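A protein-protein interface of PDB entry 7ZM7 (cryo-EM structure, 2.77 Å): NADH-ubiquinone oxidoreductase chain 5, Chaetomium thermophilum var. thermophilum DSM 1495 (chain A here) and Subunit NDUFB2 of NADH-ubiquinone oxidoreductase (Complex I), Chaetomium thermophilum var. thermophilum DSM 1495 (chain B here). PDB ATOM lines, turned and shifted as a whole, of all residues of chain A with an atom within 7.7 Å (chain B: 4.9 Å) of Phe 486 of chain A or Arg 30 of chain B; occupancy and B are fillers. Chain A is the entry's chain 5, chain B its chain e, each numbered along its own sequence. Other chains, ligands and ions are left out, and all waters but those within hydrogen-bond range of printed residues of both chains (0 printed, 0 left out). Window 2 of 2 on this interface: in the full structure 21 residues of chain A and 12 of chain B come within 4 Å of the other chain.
Of the printed residues of chain A, Arg 30 of chain B touches Phe 385 (3.6 Å), Tyr 390 (3.6 Å) and Phe 486 (3.4 Å). Printed residues of chain B within 4 Å of Phe 483 of chain A: Trp 26. Of the printed residues of chain B, Met 386 of chain A touches Ile 27. Printed residues of chain A within 4 Å of Trp 26 of chain B: Phe 385 (3.4 Å), Phe 483 (3.7 Å) and Phe 486 (3.6 Å). Tyr 29 of chain B touches none of the printed residues of chain A. The nearest residue of chain B that does not touch Phe 486 of chain A is Asp 34 of chain B (4.4 Å). The nearest residue of chain A that does not touch Arg 30 of chain B is Pro 384 of chain A (6.8 Å). The nearest printed residue of chain B that does not touch Tyr 390 of chain A is Asp 34 of chain B (4.9 Å).
Among the printed residues, merely in contact across the chains: Phe 486 of chain A with Arg 30 of chain B, Met 386 of chain A with Ile 27 of chain B, Phe 385 of chain A with Trp 26 of chain B, Phe 385 of chain A with Arg 30 of chain B, Tyr 390 of chain A with Arg 30 of chain B, Phe 486 of chain A with Trp 26 of chain B, Phe 483 of chain A with Trp 26 of chain B, Pro 384 of chain A with Ile 27 of chain B and Phe 385 of chain A with Ala 31 of chain B.
The backbone carbonyl oxygen (O) of Arg 30 of chain B sits at hydrogen-bond distance from the backbone NH (N) of Gly 35 of chain B (3.5 Å). The side-chain carboxylate (OD2) of Asp 34 of chain B lies within salt-bridge range of the guanidinium group (NH2) of Arg 30 of chain B, at 2.8 Å.
Of the 19 printed residues of chain A, 6 touch a printed residue of chain B. Hydrophobic or aromatic side chains of chain A within 4 Å of the printed part of chain B: Phe 385, Met 386, Tyr 390, Phe 483 and Phe 486. Of the 10 printed residues of chain B, 4 touch a printed residue of chain A. Hydrophobic or aromatic side chains of chain B within 4 Å of the printed part of chain A: Trp 26, Ile 27 and Ala 31. Among the printed residues, no Asp or Glu carboxylate lies within 4 Å of a Lys or Arg side-chain nitrogen of the other chain.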
ATOM      1  N   PHE A 327      10.976  17.212 -13.259  1.00  0.00           N
ATOM      2  CA  PHE A 327      12.177  17.262 -14.077  1.00  0.00           C
ATOM      3  C   PHE A 327      13.079  16.064 -13.813  1.00  0.00           C
ATOM      4  O   PHE A 327      13.551  15.413 -14.748  1.00  0.00           O
ATOM      5  CB  PHE A 327      12.911  18.563 -13.812  1.00  0.00           C
ATOM      6  CG  PHE A 327      13.947  18.889 -14.825  1.00  0.00           C
ATOM      7  CD1 PHE A 327      13.669  18.794 -16.171  1.00  0.00           C
ATOM      8  CD2 PHE A 327      15.178  19.353 -14.436  1.00  0.00           C
ATOM      9  CE1 PHE A 327      14.610  19.119 -17.101  1.00  0.00           C
ATOM     10  CE2 PHE A 327      16.127  19.684 -15.368  1.00  0.00           C
ATOM     11  CZ  PHE A 327      15.847  19.568 -16.695  1.00  0.00           C
ATOM     12  N   ASN A 331      14.070  13.096 -16.527  1.00  0.00           N
ATOM     13  CA  ASN A 331      15.495  12.908 -16.776  1.00  0.00           C
ATOM     14  C   ASN A 331      15.954  11.515 -16.389  1.00  0.00           C
ATOM     15  O   ASN A 331      16.755  10.902 -17.097  1.00  0.00           O
ATOM     16  CB  ASN A 331      16.304  13.927 -15.989  1.00  0.00           C
ATOM     17  CG  ASN A 331      16.245  15.289 -16.582  1.00  0.00           C
ATOM     18  OD1 ASN A 331      15.488  15.543 -17.513  1.00  0.00           O
ATOM     19  ND2 ASN A 331      17.057  16.186 -16.058  1.00  0.00           N
ATOM     20  N   PRO A 384      28.780  17.380 -13.685  1.00  0.00           N
ATOM     21  CA  PRO A 384      28.354  18.690 -14.184  1.00  0.00           C
ATOM     22  C   PRO A 384      27.994  18.640 -15.659  1.00  0.00           C
ATOM     23  O   PRO A 384      28.637  17.950 -16.452  1.00  0.00           O
ATOM     24  CB  PRO A 384      29.576  19.580 -13.933  1.00  0.00           C
ATOM     25  CG  PRO A 384      30.546  18.759 -13.124  1.00  0.00           C
ATOM     26  CD  PRO A 384      29.888  17.487 -12.728  1.00  0.00           C
ATOM     27  N   PHE A 385      26.916  19.341 -16.009  1.00  0.00           N
ATOM     28  CA  PHE A 385      26.452  19.521 -17.381  1.00  0.00           C
ATOM     29  C   PHE A 385      25.972  18.228 -18.027  1.00  0.00           C
ATOM     30  O   PHE A 385      25.957  18.114 -19.256  1.00  0.00           O
ATOM     31  CB  PHE A 385      27.540  20.180 -18.230  1.00  0.00           C
ATOM     32  CG  PHE A 385      28.210  21.327 -17.542  1.00  0.00           C
ATOM     33  CD1 PHE A 385      27.517  22.491 -17.287  1.00  0.00           C
ATOM     34  CD2 PHE A 385      29.521  21.230 -17.123  1.00  0.00           C
ATOM     35  CE1 PHE A 385      28.127  23.548 -16.646  1.00  0.00           C
ATOM     36  CE2 PHE A 385      30.136  22.282 -16.482  1.00  0.00           C
ATOM     37  CZ  PHE A 385      29.439  23.441 -16.241  1.00  0.00           C
ATOM     38  N   MET A 386      25.556  17.260 -17.224  1.00  0.00           N
ATOM     39  CA  MET A 386      24.803  16.107 -17.692  1.00  0.00           C
ATOM     40  C   MET A 386      23.321  16.325 -17.458  1.00  0.00           C
ATOM     41  O   MET A 386      22.902  17.288 -16.815  1.00  0.00           O
ATOM     42  CB  MET A 386      25.271  14.828 -16.997  1.00  0.00           C
ATOM     43  CG  MET A 386      26.677  14.392 -17.323  1.00  0.00           C
ATOM     44  SD  MET A 386      26.763  14.030 -19.081  1.00  0.00           S
ATOM     45  CE  MET A 386      27.561  15.473 -19.751  1.00  0.00           C
ATOM     46  N   THR A 387      22.517  15.412 -17.999  1.00  0.00           N
ATOM     47  CA  THR A 387      21.075  15.524 -17.831  1.00  0.00           C
ATOM     48  C   THR A 387      20.696  15.403 -16.365  1.00  0.00           C
ATOM     49  O   THR A 387      19.676  15.947 -15.933  1.00  0.00           O
ATOM     50  CB  THR A 387      20.370  14.482 -18.695  1.00  0.00           C
ATOM     51  OG1 THR A 387      20.585  14.809 -20.068  1.00  0.00           O
ATOM     52  CG2 THR A 387      18.889  14.470 -18.461  1.00  0.00           C
ATOM     53  N   GLY A 388      21.533  14.737 -15.573  1.00  0.00           N
ATOM     54  CA  GLY A 388      21.272  14.653 -14.151  1.00  0.00           C
ATOM     55  C   GLY A 388      21.713  15.876 -13.374  1.00  0.00           C
ATOM     56  O   GLY A 388      21.187  16.146 -12.291  1.00  0.00           O
ATOM     57  N   TYR A 390      21.239  18.974 -14.074  1.00  0.00           N
ATOM     58  CA  TYR A 390      20.217  20.002 -14.042  1.00  0.00           C
ATOM     59  C   TYR A 390      18.995  19.599 -13.234  1.00  0.00           C
ATOM     60  O   TYR A 390      18.123  20.445 -13.011  1.00  0.00           O
ATOM     61  CB  TYR A 390      19.812  20.373 -15.461  1.00  0.00           C
ATOM     62  CG  TYR A 390      20.894  21.109 -16.204  1.00  0.00           C
ATOM     63  CD1 TYR A 390      21.324  22.355 -15.777  1.00  0.00           C
ATOM     64  CD2 TYR A 390      21.491  20.559 -17.325  1.00  0.00           C
ATOM     65  CE1 TYR A 390      22.316  23.032 -16.445  1.00  0.00           C
ATOM     66  CE2 TYR A 390      22.485  21.229 -18.001  1.00  0.00           C
ATOM     67  CZ  TYR A 390      22.893  22.467 -17.558  1.00  0.00           C
ATOM     68  OH  TYR A 390      23.884  23.140 -18.230  1.00  0.00           O
ATOM     69  N   PHE A 480      20.088  11.105 -25.419  1.00  0.00           N
ATOM     70  CA  PHE A 480      19.245  11.782 -24.437  1.00  0.00           C
ATOM     71  C   PHE A 480      20.017  12.093 -23.165  1.00  0.00           C
ATOM     72  O   PHE A 480      20.015  13.233 -22.695  1.00  0.00           O
ATOM     73  CB  PHE A 480      18.028  10.933 -24.102  1.00  0.00           C
ATOM     74  CG  PHE A 480      16.877  11.140 -25.016  1.00  0.00           C
ATOM     75  CD1 PHE A 480      16.021  12.203 -24.828  1.00  0.00           C
ATOM     76  CD2 PHE A 480      16.630  10.263 -26.052  1.00  0.00           C
ATOM     77  CE1 PHE A 480      14.946  12.400 -25.666  1.00  0.00           C
ATOM     78  CE2 PHE A 480      15.556  10.453 -26.895  1.00  0.00           C
ATOM     79  CZ  PHE A 480      14.713  11.524 -26.701  1.00  0.00           C
ATOM     80  N   ILE A 482      22.638  12.992 -22.378  1.00  0.00           N
ATOM     81  CA  ILE A 482      23.600  14.080 -22.448  1.00  0.00           C
ATOM     82  C   ILE A 482      22.910  15.428 -22.583  1.00  0.00           C
ATOM     83  O   ILE A 482      23.112  16.323 -21.765  1.00  0.00           O
ATOM     84  CB  ILE A 482      24.584  13.840 -23.614  1.00  0.00           C
ATOM     85  CG1 ILE A 482      25.341  12.533 -23.415  1.00  0.00           C
ATOM     86  CG2 ILE A 482      25.578  14.966 -23.687  1.00  0.00           C
ATOM     87  CD1 ILE A 482      26.302  12.571 -22.259  1.00  0.00           C
ATOM     88  N   PHE A 483      22.064  15.585 -23.600  1.00  0.00           N
ATOM     89  CA  PHE A 483      21.535  16.890 -23.956  1.00  0.00           C
ATOM     90  C   PHE A 483      20.186  17.218 -23.340  1.00  0.00           C
ATOM     91  O   PHE A 483      19.782  18.383 -23.381  1.00  0.00           O
ATOM     92  CB  PHE A 483      21.401  17.011 -25.481  1.00  0.00           C
ATOM     93  CG  PHE A 483      22.711  17.051 -26.206  1.00  0.00           C
ATOM     94  CD1 PHE A 483      23.888  17.289 -25.527  1.00  0.00           C
ATOM     95  CD2 PHE A 483      22.763  16.849 -27.572  1.00  0.00           C
ATOM     96  CE1 PHE A 483      25.090  17.327 -26.196  1.00  0.00           C
ATOM     97  CE2 PHE A 483      23.963  16.883 -28.245  1.00  0.00           C
ATOM     98  CZ  PHE A 483      25.129  17.121 -27.556  1.00  0.00           C
ATOM     99  N   PHE A 484      19.479  16.241 -22.779  1.00  0.00           N
ATOM    100  CA  PHE A 484      18.076  16.479 -22.484  1.00  0.00           C
ATOM    101  C   PHE A 484      17.901  17.423 -21.304  1.00  0.00           C
ATOM    102  O   PHE A 484      16.938  18.197 -21.267  1.00  0.00           O
ATOM    103  CB  PHE A 484      17.359  15.157 -22.238  1.00  0.00           C
ATOM    104  CG  PHE A 484      15.904  15.310 -21.982  1.00  0.00           C
ATOM    105  CD1 PHE A 484      15.044  15.573 -23.024  1.00  0.00           C
ATOM    106  CD2 PHE A 484      15.394  15.220 -20.707  1.00  0.00           C
ATOM    107  CE1 PHE A 484      13.696  15.726 -22.804  1.00  0.00           C
ATOM    108  CE2 PHE A 484      14.041  15.378 -20.475  1.00  0.00           C
ATOM    109  CZ  PHE A 484      13.192  15.630 -21.529  1.00  0.00           C
ATOM    110  N   GLY A 485      18.811  17.377 -20.331  1.00  0.00           N
ATOM    111  CA  GLY A 485      18.690  18.269 -19.193  1.00  0.00           C
ATOM    112  C   GLY A 485      18.771  19.726 -19.598  1.00  0.00           C
ATOM    113  O   GLY A 485      17.916  20.533 -19.235  1.00  0.00           O
ATOM    114  N   PHE A 486      19.779  20.070 -20.395  1.00  0.00           N
ATOM    115  CA  PHE A 486      19.981  21.465 -20.763  1.00  0.00           C
ATOM    116  C   PHE A 486      18.870  21.979 -21.662  1.00  0.00           C
ATOM    117  O   PHE A 486      18.542  23.168 -21.620  1.00  0.00           O
ATOM    118  CB  PHE A 486      21.335  21.632 -21.447  1.00  0.00           C
ATOM    119  CG  PHE A 486      21.616  23.030 -21.896  1.00  0.00           C
ATOM    120  CD1 PHE A 486      22.023  23.993 -20.994  1.00  0.00           C
ATOM    121  CD2 PHE A 486      21.482  23.380 -23.225  1.00  0.00           C
ATOM    122  CE1 PHE A 486      22.284  25.279 -21.405  1.00  0.00           C
ATOM    123  CE2 PHE A 486      21.743  24.664 -23.645  1.00  0.00           C
ATOM    124  CZ  PHE A 486      22.145  25.615 -22.733  1.00  0.00           C
ATOM    125  N   ILE A 487      18.276  21.111 -22.477  1.00  0.00           N
ATOM    126  CA  ILE A 487      17.349  21.588 -23.487  1.00  0.00           C
ATOM    127  C   ILE A 487      15.977  21.905 -22.911  1.00  0.00           C
ATOM    128  O   ILE A 487      15.280  22.773 -23.441  1.00  0.00           O
ATOM    129  CB  ILE A 487      17.271  20.566 -24.634  1.00  0.00           C
ATOM    130  CG1 ILE A 487      16.797  21.250 -25.913  1.00  0.00           C
ATOM    131  CG2 ILE A 487      16.384  19.397 -24.267  1.00  0.00           C
ATOM    132  CD1 ILE A 487      17.660  22.407 -26.319  1.00  0.00           C
ATOM    133  N   THR A 488      15.574  21.238 -21.832  1.00  0.00           N
ATOM    134  CA  THR A 488      14.276  21.452 -21.210  1.00  0.00           C
ATOM    135  C   THR A 488      14.383  22.083 -19.832  1.00  0.00           C
ATOM    136  O   THR A 488      13.373  22.179 -19.124  1.00  0.00           O
ATOM    137  CB  THR A 488      13.513  20.129 -21.129  1.00  0.00           C
ATOM    138  OG1 THR A 488      14.251  19.202 -20.327  1.00  0.00           O
ATOM    139  CG2 THR A 488      13.290  19.546 -22.508  1.00  0.00           C
ATOM    140  N   LYS A 489      15.570  22.542 -19.442  1.00  0.00           N
ATOM    141  CA  LYS A 489      15.755  23.064 -18.093  1.00  0.00           C
ATOM    142  C   LYS A 489      14.987  24.359 -17.881  1.00  0.00           C
ATOM    143  O   LYS A 489      14.880  24.838 -16.749  1.00  0.00           O
ATOM    144  CB  LYS A 489      17.237  23.278 -17.810  1.00  0.00           C
ATOM    145  CG  LYS A 489      17.755  24.647 -18.204  1.00  0.00           C
ATOM    146  CD  LYS A 489      19.226  24.799 -17.853  1.00  0.00           C
ATOM    147  CE  LYS A 489      19.724  26.201 -18.146  1.00  0.00           C
ATOM    148  NZ  LYS A 489      19.133  27.203 -17.220  1.00  0.00           N
ATOM    149  N   ASP A 490      14.478  24.956 -18.947  1.00  0.00           N
ATOM    150  CA  ASP A 490      13.658  26.143 -18.796  1.00  0.00           C
ATOM    151  C   ASP A 490      12.182  25.802 -18.714  1.00  0.00           C
ATOM    152  O   ASP A 490      11.441  26.446 -17.970  1.00  0.00           O
ATOM    153  CB  ASP A 490      13.926  27.094 -19.955  1.00  0.00           C
ATOM    154  CG  ASP A 490      13.149  28.363 -19.848  1.00  0.00           C
ATOM    155  OD1 ASP A 490      13.133  28.958 -18.758  1.00  0.00           O
ATOM    156  OD2 ASP A 490      12.556  28.762 -20.861  1.00  0.00           O
ATOM    157  N   ILE A 491      11.754  24.781 -19.452  1.00  0.00           N
ATOM    158  CA  ILE A 491      10.370  24.336 -19.419  1.00  0.00           C
ATOM    159  C   ILE A 491       9.956  23.988 -18.001  1.00  0.00           C
ATOM    160  O   ILE A 491       8.839  24.292 -17.571  1.00  0.00           O
ATOM    161  CB  ILE A 491      10.192  23.140 -20.374  1.00  0.00           C
ATOM    162  CG1 ILE A 491      10.479  23.568 -21.800  1.00  0.00           C
ATOM    163  CG2 ILE A 491       8.822  22.517 -20.244  1.00  0.00           C
ATOM    164  CD1 ILE A 491      10.587  22.438 -22.758  1.00  0.00           C
ATOM    165  N   TRP B  26      30.741  18.828 -25.095  1.00  0.00           N
ATOM    166  CA  TRP B  26      29.653  19.493 -24.404  1.00  0.00           C
ATOM    167  C   TRP B  26      30.118  19.971 -23.040  1.00  0.00           C
ATOM    168  O   TRP B  26      29.673  21.014 -22.552  1.00  0.00           O
ATOM    169  CB  TRP B  26      28.471  18.539 -24.278  1.00  0.00           C
ATOM    170  CG  TRP B  26      27.256  19.168 -23.722  1.00  0.00           C
ATOM    171  CD1 TRP B  26      26.669  18.899 -22.529  1.00  0.00           C
ATOM    172  CD2 TRP B  26      26.464  20.178 -24.343  1.00  0.00           C
ATOM    173  NE1 TRP B  26      25.557  19.683 -22.363  1.00  0.00           N
ATOM    174  CE2 TRP B  26      25.411  20.478 -23.466  1.00  0.00           C
ATOM    175  CE3 TRP B  26      26.545  20.860 -25.556  1.00  0.00           C
ATOM    176  CZ2 TRP B  26      24.448  21.431 -23.760  1.00  0.00           C
ATOM    177  CZ3 TRP B  26      25.587  21.805 -25.847  1.00  0.00           C
ATOM    178  CH2 TRP B  26      24.552  22.083 -24.954  1.00  0.00           C
ATOM    179  N   ILE B  27      31.024  19.217 -22.420  1.00  0.00           N
ATOM    180  CA  ILE B  27      31.505  19.546 -21.084  1.00  0.00           C
ATOM    181  C   ILE B  27      32.249  20.868 -21.085  1.00  0.00           C
ATOM    182  O   ILE B  27      31.851  21.822 -20.409  1.00  0.00           O
ATOM    183  CB  ILE B  27      32.388  18.411 -20.545  1.00  0.00           C
ATOM    184  CG1 ILE B  27      31.586  17.132 -20.484  1.00  0.00           C
ATOM    185  CG2 ILE B  27      32.939  18.762 -19.180  1.00  0.00           C
ATOM    186  CD1 ILE B  27      30.443  17.272 -19.577  1.00  0.00           C
ATOM    187  N   PHE B  28      33.332  20.950 -21.843  1.00  0.00           N
ATOM    188  CA  PHE B  28      34.103  22.184 -21.838  1.00  0.00           C
ATOM    189  C   PHE B  28      33.323  23.329 -22.460  1.00  0.00           C
ATOM    190  O   PHE B  28      33.448  24.473 -22.019  1.00  0.00           O
ATOM    191  CB  PHE B  28      35.443  21.972 -22.532  1.00  0.00           C
ATOM    192  CG  PHE B  28      36.221  20.814 -21.990  1.00  0.00           C
ATOM    193  CD1 PHE B  28      35.990  19.531 -22.429  1.00  0.00           C
ATOM    194  CD2 PHE B  28      37.194  21.021 -21.029  1.00  0.00           C
ATOM    195  CE1 PHE B  28      36.707  18.477 -21.930  1.00  0.00           C
ATOM    196  CE2 PHE B  28      37.916  19.967 -20.523  1.00  0.00           C
ATOM    197  CZ  PHE B  28      37.669  18.690 -20.977  1.00  0.00           C
ATOM    198  N   TYR B  29      32.493  23.050 -23.461  1.00  0.00           N
ATOM    199  CA  TYR B  29      31.716  24.133 -24.043  1.00  0.00           C
ATOM    200  C   TYR B  29      30.758  24.723 -23.025  1.00  0.00           C
ATOM    201  O   TYR B  29      30.542  25.938 -22.996  1.00  0.00           O
ATOM    202  CB  TYR B  29      30.948  23.665 -25.269  1.00  0.00           C
ATOM    203  CG  TYR B  29      30.231  24.803 -25.942  1.00  0.00           C
ATOM    204  CD1 TYR B  29      30.937  25.764 -26.645  1.00  0.00           C
ATOM    205  CD2 TYR B  29      28.858  24.935 -25.850  1.00  0.00           C
ATOM    206  CE1 TYR B  29      30.292  26.812 -27.256  1.00  0.00           C
ATOM    207  CE2 TYR B  29      28.204  25.980 -26.456  1.00  0.00           C
ATOM    208  CZ  TYR B  29      28.926  26.918 -27.157  1.00  0.00           C
ATOM    209  OH  TYR B  29      28.280  27.967 -27.766  1.00  0.00           O
ATOM    210  N   ARG B  30      30.157  23.877 -22.192  1.00  0.00           N
ATOM    211  CA  ARG B  30      29.300  24.394 -21.136  1.00  0.00           C
ATOM    212  C   ARG B  30      30.127  24.963 -19.993  1.00  0.00           C
ATOM    213  O   ARG B  30      29.764  25.989 -19.407  1.00  0.00           O
ATOM    214  CB  ARG B  30      28.360  23.298 -20.646  1.00  0.00           C
ATOM    215  CG  ARG B  30      27.214  23.030 -21.599  1.00  0.00           C
ATOM    216  CD  ARG B  30      25.949  23.682 -21.105  1.00  0.00           C
ATOM    217  NE  ARG B  30      25.999  25.135 -21.201  1.00  0.00           N
ATOM    218  CZ  ARG B  30      25.757  25.816 -22.314  1.00  0.00           C
ATOM    219  NH1 ARG B  30      25.442  25.173 -23.429  1.00  0.00           N
ATOM    220  NH2 ARG B  30      25.819  27.138 -22.311  1.00  0.00           N
ATOM    221  N   ALA B  31      31.249  24.320 -19.674  1.00  0.00           N
ATOM    222  CA  ALA B  31      32.137  24.854 -18.650  1.00  0.00           C
ATOM    223  C   ALA B  31      32.749  26.176 -19.087  1.00  0.00           C
ATOM    224  O   ALA B  31      32.900  27.093 -18.276  1.00  0.00           O
ATOM    225  CB  ALA B  31      33.230  23.841 -18.320  1.00  0.00           C
ATOM    226  N   LYS B  32      33.115  26.295 -20.360  1.00  0.00           N
ATOM    227  CA  LYS B  32      33.680  27.557 -20.821  1.00  0.00           C
ATOM    228  C   LYS B  32      32.636  28.667 -20.828  1.00  0.00           C
ATOM    229  O   LYS B  32      32.959  29.821 -20.528  1.00  0.00           O
ATOM    230  CB  LYS B  32      34.292  27.391 -22.210  1.00  0.00           C
ATOM    231  CG  LYS B  32      34.682  28.704 -22.869  1.00  0.00           C
ATOM    232  CD  LYS B  32      35.555  28.484 -24.088  1.00  0.00           C
ATOM    233  CE  LYS B  32      35.665  29.752 -24.911  1.00  0.00           C
ATOM    234  NZ  LYS B  32      34.336  30.193 -25.414  1.00  0.00           N
ATOM    235  N   LYS B  33      31.384  28.342 -21.145  1.00  0.00           N
ATOM    236  CA  LYS B  33      30.362  29.366 -21.314  1.00  0.00           C
ATOM    237  C   LYS B  33      29.604  29.670 -20.028  1.00  0.00           C
ATOM    238  O   LYS B  33      29.309  30.836 -19.749  1.00  0.00           O
ATOM    239  CB  LYS B  33      29.382  28.944 -22.410  1.00  0.00           C
ATOM    240  CG  LYS B  33      28.323  29.974 -22.732  1.00  0.00           C
ATOM    241  CD  LYS B  33      27.432  29.495 -23.864  1.00  0.00           C
ATOM    242  CE  LYS B  33      26.419  30.554 -24.263  1.00  0.00           C
ATOM    243  NZ  LYS B  33      25.419  30.789 -23.186  1.00  0.00           N
ATOM    244  N   ASP B  34      29.283  28.651 -19.231  1.00  0.00           N
ATOM    245  CA  ASP B  34      28.521  28.847 -18.006  1.00  0.00           C
ATOM    246  C   ASP B  34      29.317  28.552 -16.745  1.00  0.00           C
ATOM    247  O   ASP B  34      28.760  28.643 -15.646  1.00  0.00           O
ATOM    248  CB  ASP B  34      27.254  27.981 -18.014  1.00  0.00           C
ATOM    249  CG  ASP B  34      26.241  28.444 -19.036  1.00  0.00           C
ATOM    250  OD1 ASP B  34      26.212  29.656 -19.333  1.00  0.00           O
ATOM    251  OD2 ASP B  34      25.470  27.599 -19.537  1.00  0.00           O
ATOM    252  N   GLY B  35      30.591  28.199 -16.867  1.00  0.00           N
ATOM    253  CA  GLY B  35      31.417  27.904 -15.722  1.00  0.00           C
ATOM    254  C   GLY B  35      31.570  29.048 -14.739  1.00  0.00           C
ATOM    255  O   GLY B  35      31.417  28.859 -13.529  1.00  0.00           O
